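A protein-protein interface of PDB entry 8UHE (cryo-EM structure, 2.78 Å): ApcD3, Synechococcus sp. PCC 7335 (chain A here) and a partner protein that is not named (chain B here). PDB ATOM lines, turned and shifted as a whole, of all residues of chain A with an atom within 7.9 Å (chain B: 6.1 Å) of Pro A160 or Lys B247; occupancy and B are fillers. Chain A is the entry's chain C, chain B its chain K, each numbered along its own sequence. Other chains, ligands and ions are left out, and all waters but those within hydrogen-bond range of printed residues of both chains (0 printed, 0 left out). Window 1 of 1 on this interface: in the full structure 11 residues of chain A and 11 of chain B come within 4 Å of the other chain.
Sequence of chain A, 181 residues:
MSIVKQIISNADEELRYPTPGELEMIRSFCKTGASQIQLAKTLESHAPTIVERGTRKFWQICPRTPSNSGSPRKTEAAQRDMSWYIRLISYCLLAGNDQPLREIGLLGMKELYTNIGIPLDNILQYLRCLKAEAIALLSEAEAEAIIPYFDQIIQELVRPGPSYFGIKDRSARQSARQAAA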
ATOM      1  N   LYS A 110      22.280   7.641  12.237  1.00  0.00           N
ATOM      2  CA  LYS A 110      21.722   7.046  13.449  1.00  0.00           C
ATOM      3  C   LYS A 110      22.165   5.600  13.605  1.00  0.00           C
ATOM      4  O   LYS A 110      22.580   5.176  14.690  1.00  0.00           O
ATOM      5  CB  LYS A 110      20.195   7.121  13.407  1.00  0.00           C
ATOM      6  CG  LYS A 110      19.637   8.514  13.536  1.00  0.00           C
ATOM      7  CD  LYS A 110      18.444   8.538  14.466  1.00  0.00           C
ATOM      8  CE  LYS A 110      17.313   7.714  13.894  1.00  0.00           C
ATOM      9  NZ  LYS A 110      16.431   8.557  13.052  1.00  0.00           N
ATOM     10  N   GLU A 111      22.085   4.827  12.522  1.00  0.00           N
ATOM     11  CA  GLU A 111      22.508   3.434  12.578  1.00  0.00           C
ATOM     12  C   GLU A 111      24.019   3.320  12.733  1.00  0.00           C
ATOM     13  O   GLU A 111      24.505   2.396  13.402  1.00  0.00           O
ATOM     14  CB  GLU A 111      22.003   2.693  11.345  1.00  0.00           C
ATOM     15  CG  GLU A 111      22.450   3.296  10.047  1.00  0.00           C
ATOM     16  CD  GLU A 111      21.332   3.378   9.037  1.00  0.00           C
ATOM     17  OE1 GLU A 111      21.369   2.612   8.058  1.00  0.00           O
ATOM     18  OE2 GLU A 111      20.422   4.215   9.217  1.00  0.00           O
ATOM     19  N   THR A 114      24.489   3.981  16.546  1.00  0.00           N
ATOM     20  CA  THR A 114      23.990   2.875  17.357  1.00  0.00           C
ATOM     21  C   THR A 114      24.851   1.634  17.188  1.00  0.00           C
ATOM     22  O   THR A 114      24.909   0.796  18.093  1.00  0.00           O
ATOM     23  CB  THR A 114      22.538   2.546  17.016  1.00  0.00           C
ATOM     24  OG1 THR A 114      22.408   2.359  15.604  1.00  0.00           O
ATOM     25  CG2 THR A 114      21.615   3.662  17.467  1.00  0.00           C
ATOM     26  N   PRO A 119      24.978   6.965  22.539  1.00  0.00           N
ATOM     27  CA  PRO A 119      23.545   7.278  22.593  1.00  0.00           C
ATOM     28  C   PRO A 119      23.228   8.525  21.782  1.00  0.00           C
ATOM     29  O   PRO A 119      23.934   9.532  21.853  1.00  0.00           O
ATOM     30  CB  PRO A 119      23.283   7.499  24.088  1.00  0.00           C
ATOM     31  CG  PRO A 119      24.437   6.856  24.786  1.00  0.00           C
ATOM     32  CD  PRO A 119      25.605   7.001  23.870  1.00  0.00           C
ATOM     33  N   LEU A 120      22.147   8.449  21.005  1.00  0.00           N
ATOM     34  CA  LEU A 120      21.823   9.529  20.084  1.00  0.00           C
ATOM     35  C   LEU A 120      21.122  10.704  20.757  1.00  0.00           C
ATOM     36  O   LEU A 120      21.124  11.803  20.195  1.00  0.00           O
ATOM     37  CB  LEU A 120      20.952   9.006  18.946  1.00  0.00           C
ATOM     38  CG  LEU A 120      21.143   7.587  18.428  1.00  0.00           C
ATOM     39  CD1 LEU A 120      19.900   7.163  17.675  1.00  0.00           C
ATOM     40  CD2 LEU A 120      22.357   7.492  17.546  1.00  0.00           C
ATOM     41  N   ASP A 121      20.512  10.504  21.930  1.00  0.00           N
ATOM     42  CA  ASP A 121      19.945  11.641  22.651  1.00  0.00           C
ATOM     43  C   ASP A 121      21.041  12.544  23.194  1.00  0.00           C
ATOM     44  O   ASP A 121      20.907  13.775  23.185  1.00  0.00           O
ATOM     45  CB  ASP A 121      19.043  11.171  23.789  1.00  0.00           C
ATOM     46  CG  ASP A 121      18.407  12.330  24.538  1.00  0.00           C
ATOM     47  OD1 ASP A 121      19.000  12.806  25.530  1.00  0.00           O
ATOM     48  OD2 ASP A 121      17.315  12.775  24.127  1.00  0.00           O
ATOM     49  N   ASN A 122      22.132  11.949  23.674  1.00  0.00           N
ATOM     50  CA  ASN A 122      23.281  12.742  24.087  1.00  0.00           C
ATOM     51  C   ASN A 122      23.906  13.453  22.894  1.00  0.00           C
ATOM     52  O   ASN A 122      24.404  14.578  23.027  1.00  0.00           O
ATOM     53  CB  ASN A 122      24.296  11.849  24.798  1.00  0.00           C
ATOM     54  CG  ASN A 122      23.696  11.135  25.994  1.00  0.00           C
ATOM     55  OD1 ASN A 122      22.747  11.625  26.608  1.00  0.00           O
ATOM     56  ND2 ASN A 122      24.246   9.976  26.333  1.00  0.00           N
ATOM     57  N   ILE A 123      23.867  12.817  21.717  1.00  0.00           N
ATOM     58  CA  ILE A 123      24.303  13.471  20.493  1.00  0.00           C
ATOM     59  C   ILE A 123      23.429  14.666  20.215  1.00  0.00           C
ATOM     60  O   ILE A 123      23.950  15.757  20.001  1.00  0.00           O
ATOM     61  CB  ILE A 123      24.324  12.479  19.317  1.00  0.00           C
ATOM     62  CG1 ILE A 123      25.380  11.411  19.558  1.00  0.00           C
ATOM     63  CG2 ILE A 123      24.614  13.149  18.008  1.00  0.00           C
ATOM     64  CD1 ILE A 123      25.629  10.523  18.364  1.00  0.00           C
ATOM     65  N   LEU A 124      22.108  14.511  20.347  1.00  0.00           N
ATOM     66  CA  LEU A 124      21.170  15.615  20.143  1.00  0.00           C
ATOM     67  C   LEU A 124      21.456  16.776  21.088  1.00  0.00           C
ATOM     68  O   LEU A 124      21.463  17.942  20.674  1.00  0.00           O
ATOM     69  CB  LEU A 124      19.746  15.097  20.340  1.00  0.00           C
ATOM     70  CG  LEU A 124      18.625  16.093  20.623  1.00  0.00           C
ATOM     71  CD1 LEU A 124      18.126  16.721  19.335  1.00  0.00           C
ATOM     72  CD2 LEU A 124      17.497  15.393  21.360  1.00  0.00           C
ATOM     73  N   GLN A 155      17.617  18.030  13.610  1.00  0.00           N
ATOM     74  CA  GLN A 155      16.252  17.541  13.435  1.00  0.00           C
ATOM     75  C   GLN A 155      16.177  16.051  13.118  1.00  0.00           C
ATOM     76  O   GLN A 155      15.090  15.470  13.196  1.00  0.00           O
ATOM     77  CB  GLN A 155      15.544  18.336  12.336  1.00  0.00           C
ATOM     78  CG  GLN A 155      14.945  19.645  12.814  1.00  0.00           C
ATOM     79  CD  GLN A 155      13.885  19.443  13.870  1.00  0.00           C
ATOM     80  OE1 GLN A 155      13.064  18.533  13.771  1.00  0.00           O
ATOM     81  NE2 GLN A 155      13.902  20.287  14.895  1.00  0.00           N
ATOM     82  N   GLU A 156      17.304  15.433  12.838  1.00  0.00           N
ATOM     83  CA  GLU A 156      17.323  14.034  12.484  1.00  0.00           C
ATOM     84  C   GLU A 156      17.343  13.110  13.678  1.00  0.00           C
ATOM     85  O   GLU A 156      17.216  11.905  13.511  1.00  0.00           O
ATOM     86  CB  GLU A 156      18.558  13.776  11.660  1.00  0.00           C
ATOM     87  CG  GLU A 156      18.548  14.473  10.304  1.00  0.00           C
ATOM     88  CD  GLU A 156      17.425  14.002   9.405  1.00  0.00           C
ATOM     89  OE1 GLU A 156      17.592  12.970   8.721  1.00  0.00           O
ATOM     90  OE2 GLU A 156      16.368  14.668   9.382  1.00  0.00           O
ATOM     91  N   LEU A 157      17.441  13.650  14.886  1.00  0.00           N
ATOM     92  CA  LEU A 157      17.597  12.793  16.056  1.00  0.00           C
ATOM     93  C   LEU A 157      16.831  13.125  17.292  1.00  0.00           C
ATOM     94  O   LEU A 157      16.610  12.473  18.222  1.00  0.00           O
ATOM     95  CB  LEU A 157      19.084  12.795  16.439  1.00  0.00           C
ATOM     96  CG  LEU A 157      20.068  13.446  15.478  1.00  0.00           C
ATOM     97  CD1 LEU A 157      21.190  14.101  16.260  1.00  0.00           C
ATOM     98  CD2 LEU A 157      20.615  12.416  14.502  1.00  0.00           C
ATOM     99  N   VAL A 158      15.800  13.958  17.009  1.00  0.00           N
ATOM    100  CA  VAL A 158      14.945  14.325  18.130  1.00  0.00           C
ATOM    101  C   VAL A 158      13.707  13.515  17.958  1.00  0.00           C
ATOM    102  O   VAL A 158      12.801  13.548  18.769  1.00  0.00           O
ATOM    103  CB  VAL A 158      14.653  15.847  18.116  1.00  0.00           C
ATOM    104  CG1 VAL A 158      15.236  16.489  16.873  1.00  0.00           C
ATOM    105  CG2 VAL A 158      13.169  16.177  18.241  1.00  0.00           C
ATOM    106  N   ARG A 159      13.733  12.665  16.944  1.00  0.00           N
ATOM    107  CA  ARG A 159      12.474  12.011  16.595  1.00  0.00           C
ATOM    108  C   ARG A 159      12.017  10.666  17.128  1.00  0.00           C
ATOM    109  O   ARG A 159      11.210   9.990  16.491  1.00  0.00           O
ATOM    110  CB  ARG A 159      12.346  12.022  15.057  1.00  0.00           C
ATOM    111  CG  ARG A 159      10.961  12.451  14.607  1.00  0.00           C
ATOM    112  CD  ARG A 159      10.900  12.679  13.112  1.00  0.00           C
ATOM    113  NE  ARG A 159      10.995  14.095  12.782  1.00  0.00           N
ATOM    114  CZ  ARG A 159      10.723  14.599  11.587  1.00  0.00           C
ATOM    115  NH1 ARG A 159      10.331  13.793  10.610  1.00  0.00           N
ATOM    116  NH2 ARG A 159      10.838  15.899  11.369  1.00  0.00           N
ATOM    117  N   PRO A 160      12.522  10.261  18.285  1.00  0.00           N
ATOM    118  CA  PRO A 160      11.877   9.062  18.780  1.00  0.00           C
ATOM    119  C   PRO A 160      10.595   9.688  19.270  1.00  0.00           C
ATOM    120  O   PRO A 160       9.608   8.970  19.280  1.00  0.00           O
ATOM    121  CB  PRO A 160      12.763   8.605  19.912  1.00  0.00           C
ATOM    122  CG  PRO A 160      13.462   9.839  20.376  1.00  0.00           C
ATOM    123  CD  PRO A 160      13.626  10.698  19.155  1.00  0.00           C
ATOM    124  N   GLY A 161      10.607  10.973  19.653  1.00  0.00           N
ATOM    125  CA  GLY A 161       9.431  11.730  20.096  1.00  0.00           C
ATOM    126  C   GLY A 161       9.756  12.923  21.024  1.00  0.00           C
ATOM    127  O   GLY A 161      10.011  12.709  22.201  1.00  0.00           O
ATOM    128  N   PRO A 162       9.755  14.179  20.521  1.00  0.00           N
ATOM    129  CA  PRO A 162       9.963  15.308  21.437  1.00  0.00           C
ATOM    130  C   PRO A 162       8.979  15.302  22.664  1.00  0.00           C
ATOM    131  O   PRO A 162       7.799  15.562  22.455  1.00  0.00           O
ATOM    132  CB  PRO A 162       9.823  16.567  20.530  1.00  0.00           C
ATOM    133  CG  PRO A 162       9.538  16.052  19.162  1.00  0.00           C
ATOM    134  CD  PRO A 162       9.828  14.585  19.110  1.00  0.00           C
ATOM    135  N   SER A 163       9.461  15.054  23.882  1.00  0.00           N
ATOM    136  CA  SER A 163       8.617  14.929  25.138  1.00  0.00           C
ATOM    137  C   SER A 163       7.659  16.016  25.704  1.00  0.00           C
ATOM    138  O   SER A 163       8.110  17.127  25.969  1.00  0.00           O
ATOM    139  CB  SER A 163       9.583  14.547  26.267  1.00  0.00           C
ATOM    140  OG  SER A 163       9.480  13.184  26.603  1.00  0.00           O
ATOM    141  N   GLY B 194      10.520   0.792  19.362  1.00  0.00           N
ATOM    142  CA  GLY B 194      10.675   2.226  19.220  1.00  0.00           C
ATOM    143  C   GLY B 194      10.057   3.026  20.348  1.00  0.00           C
ATOM    144  O   GLY B 194       9.458   4.078  20.109  1.00  0.00           O
ATOM    145  N   ARG B 196      11.942   3.907  23.162  1.00  0.00           N
ATOM    146  CA  ARG B 196      13.032   4.440  23.976  1.00  0.00           C
ATOM    147  C   ARG B 196      12.879   5.937  24.211  1.00  0.00           C
ATOM    148  O   ARG B 196      13.083   6.423  25.330  1.00  0.00           O
ATOM    149  CB  ARG B 196      14.369   4.126  23.304  1.00  0.00           C
ATOM    150  CG  ARG B 196      15.572   4.818  23.910  1.00  0.00           C
ATOM    151  CD  ARG B 196      15.928   4.232  25.256  1.00  0.00           C
ATOM    152  NE  ARG B 196      17.247   4.668  25.698  1.00  0.00           N
ATOM    153  CZ  ARG B 196      18.376   4.026  25.430  1.00  0.00           C
ATOM    154  NH1 ARG B 196      18.386   2.909  24.720  1.00  0.00           N
ATOM    155  NH2 ARG B 196      19.525   4.515  25.889  1.00  0.00           N
ATOM    156  N   GLY B 197      12.496   6.679  23.179  1.00  0.00           N
ATOM    157  CA  GLY B 197      12.288   8.099  23.348  1.00  0.00           C
ATOM    158  C   GLY B 197      10.845   8.540  23.452  1.00  0.00           C
ATOM    159  O   GLY B 197      10.580   9.698  23.786  1.00  0.00           O
ATOM    160  N   ILE B 198       9.903   7.638  23.165  1.00  0.00           N
ATOM    161  CA  ILE B 198       8.496   7.934  23.424  1.00  0.00           C
ATOM    162  C   ILE B 198       8.266   8.088  24.920  1.00  0.00           C
ATOM    163  O   ILE B 198       7.689   9.079  25.384  1.00  0.00           O
ATOM    164  CB  ILE B 198       7.595   6.835  22.836  1.00  0.00           C
ATOM    165  CG1 ILE B 198       7.831   6.678  21.329  1.00  0.00           C
ATOM    166  CG2 ILE B 198       6.139   7.113  23.187  1.00  0.00           C
ATOM    167  CD1 ILE B 198       6.890   7.462  20.445  1.00  0.00           C
ATOM    168  N   GLU B 201      12.805   9.213  28.213  1.00  0.00           N
ATOM    169  CA  GLU B 201      14.209   8.873  27.965  1.00  0.00           C
ATOM    170  C   GLU B 201      15.153   9.410  29.037  1.00  0.00           C
ATOM    171  O   GLU B 201      16.358   9.138  29.000  1.00  0.00           O
ATOM    172  CB  GLU B 201      14.658   9.352  26.578  1.00  0.00           C
ATOM    173  CG  GLU B 201      15.666   8.452  25.893  1.00  0.00           C
ATOM    174  CD  GLU B 201      16.281   9.108  24.679  1.00  0.00           C
ATOM    175  OE1 GLU B 201      15.912  10.263  24.379  1.00  0.00           O
ATOM    176  OE2 GLU B 201      17.127   8.471  24.019  1.00  0.00           O
ATOM    177  N   VAL B 245      16.498  -0.781  22.422  1.00  0.00           N
ATOM    178  CA  VAL B 245      16.870  -0.354  21.079  1.00  0.00           C
ATOM    179  C   VAL B 245      16.509   1.116  20.922  1.00  0.00           C
ATOM    180  O   VAL B 245      15.357   1.514  21.134  1.00  0.00           O
ATOM    181  CB  VAL B 245      16.180  -1.223  20.020  1.00  0.00           C
ATOM    182  CG1 VAL B 245      16.275  -0.578  18.649  1.00  0.00           C
ATOM    183  CG2 VAL B 245      16.794  -2.610  20.004  1.00  0.00           C
ATOM    184  N   GLU B 246      17.495   1.933  20.555  1.00  0.00           N
ATOM    185  CA  GLU B 246      17.281   3.366  20.397  1.00  0.00           C
ATOM    186  C   GLU B 246      16.640   3.625  19.036  1.00  0.00           C
ATOM    187  O   GLU B 246      16.207   2.692  18.354  1.00  0.00           O
ATOM    188  CB  GLU B 246      18.591   4.124  20.585  1.00  0.00           C
ATOM    189  CG  GLU B 246      18.426   5.436  21.340  1.00  0.00           C
ATOM    190  CD  GLU B 246      19.742   6.140  21.567  1.00  0.00           C
ATOM    191  OE1 GLU B 246      20.745   5.704  20.968  1.00  0.00           O
ATOM    192  OE2 GLU B 246      19.776   7.126  22.333  1.00  0.00           O
ATOM    193  N   LYS B 247      16.585   4.904  18.626  1.00  0.00           N
ATOM    194  CA  LYS B 247      15.813   5.403  17.492  1.00  0.00           C
ATOM    195  C   LYS B 247      16.038   4.626  16.208  1.00  0.00           C
ATOM    196  O   LYS B 247      17.098   4.756  15.579  1.00  0.00           O
ATOM    197  CB  LYS B 247      16.173   6.845  17.209  1.00  0.00           C
ATOM    198  CG  LYS B 247      15.992   7.712  18.291  1.00  0.00           C
ATOM    199  CD  LYS B 247      16.590   9.128  18.024  1.00  0.00           C
ATOM    200  CE  LYS B 247      17.529   9.574  19.135  1.00  0.00           C
ATOM    201  NZ  LYS B 247      16.977  10.003  20.473  1.00  0.00           N
ATOM    202  N   PRO B 248      15.072   3.818  15.783  1.00  0.00           N
ATOM    203  CA  PRO B 248      15.236   3.063  14.540  1.00  0.00           C
ATOM    204  C   PRO B 248      14.660   3.812  13.349  1.00  0.00           C
ATOM    205  O   PRO B 248      13.557   4.363  13.393  1.00  0.00           O
ATOM    206  CB  PRO B 248      14.472   1.764  14.833  1.00  0.00           C
ATOM    207  CG  PRO B 248      13.489   2.120  15.955  1.00  0.00           C
ATOM    208  CD  PRO B 248      13.800   3.502  16.456  1.00  0.00           C
ATOM    209  N   SER B 249      15.429   3.818  12.264  1.00  0.00           N
ATOM    210  CA  SER B 249      15.152   4.705  11.143  1.00  0.00           C
ATOM    211  C   SER B 249      13.874   4.309  10.414  1.00  0.00           C
ATOM    212  O   SER B 249      13.654   3.136  10.096  1.00  0.00           O
ATOM    213  CB  SER B 249      16.330   4.702  10.173  1.00  0.00           C
ATOM    214  OG  SER B 249      17.550   4.540  10.873  1.00  0.00           O
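O of Lys A110 is in hydrogen-bond range of OG1 of Thr A114, at 3.0 Å.
OG1 of Thr A114 is in hydrogen-bond range of O of Glu A111, at 3.0 Å.
The backbone carbonyl oxygen (O) of Glu A156 lies within hydrogen-bond range of the side-chain amino group (NZ) of Lys A110 (3.5 Å).
The side-chain carboxylate (OE2) of Glu B201 lies within salt-bridge range of the side-chain amino group (NZ) of Lys B247, at 3.9 Å.
Among the printed residues, no Asp or Glu carboxylate lies within 4 Å of a Lys or Arg side-chain nitrogen of the other chain.
Among the printed residues, merely in contact across the chains: Pro A160 with Ile B198, Lys A110 with Lys B247, Leu A120 with Lys B247, Pro A160 with Gly B197, Pro A160 with Lys B247, Pro A119 with Glu B246 and Asp A121 with Lys B247.
The side-chain carboxylate of Glu B246 is in hydrogen-bond range of the backbone NH of Asp A121, 3.5 Å away.
The side-chain hydroxyl (OG) of Ser B249 is in hydrogen-bond range of the side-chain carboxylate (OE2) of Glu A111.
N of Leu A120 sits at hydrogen-bond distance from OE2 of Glu B246.
O of Leu A157 sits close to NZ of Lys B247 (3.4 Å).
OD2 of Asp A121 lies close to OE1 of Glu B201.
The backbone carbonyl oxygen of Gly A161 sits close to the backbone carbonyl oxygen of Gly B197.
Pro A160 touches just these residues of chain B: Gly B197, Ile B198 and Lys B247.
Of chain A, only Lys A110 (3.4 Å), Leu A120 (3.5 Å), Asp A121 (3.9 Å), Leu A157 (3.2 Å) and Pro A160 (3.5 Å) come within 4 Å of Lys B247.
Of the printed residues of chain A, Glu B201 touches Asp A121 (2.9 Å).
Printed residues of chain A within 4 Å of Gly B197: Pro A160 (3.5 Å) and Gly A161 (3.4 Å).
Of the printed residues of chain B, Leu A120 touches Glu B246 (3.0 Å) and Lys B247 (3.5 Å).
Of the printed residues of chain B, Glu A111 touches Ser B249 (3.3 Å).
Arg B196 touches none of the printed residues of chain A.
Gly B194 touches none of the printed residues of chain A.
The nearest residue of chain B that does not touch Pro A160 is Glu B201 (4.7 Å).
The nearest printed residue of chain B that does not touch Lys A110 is Ser B249 (4.4 Å).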
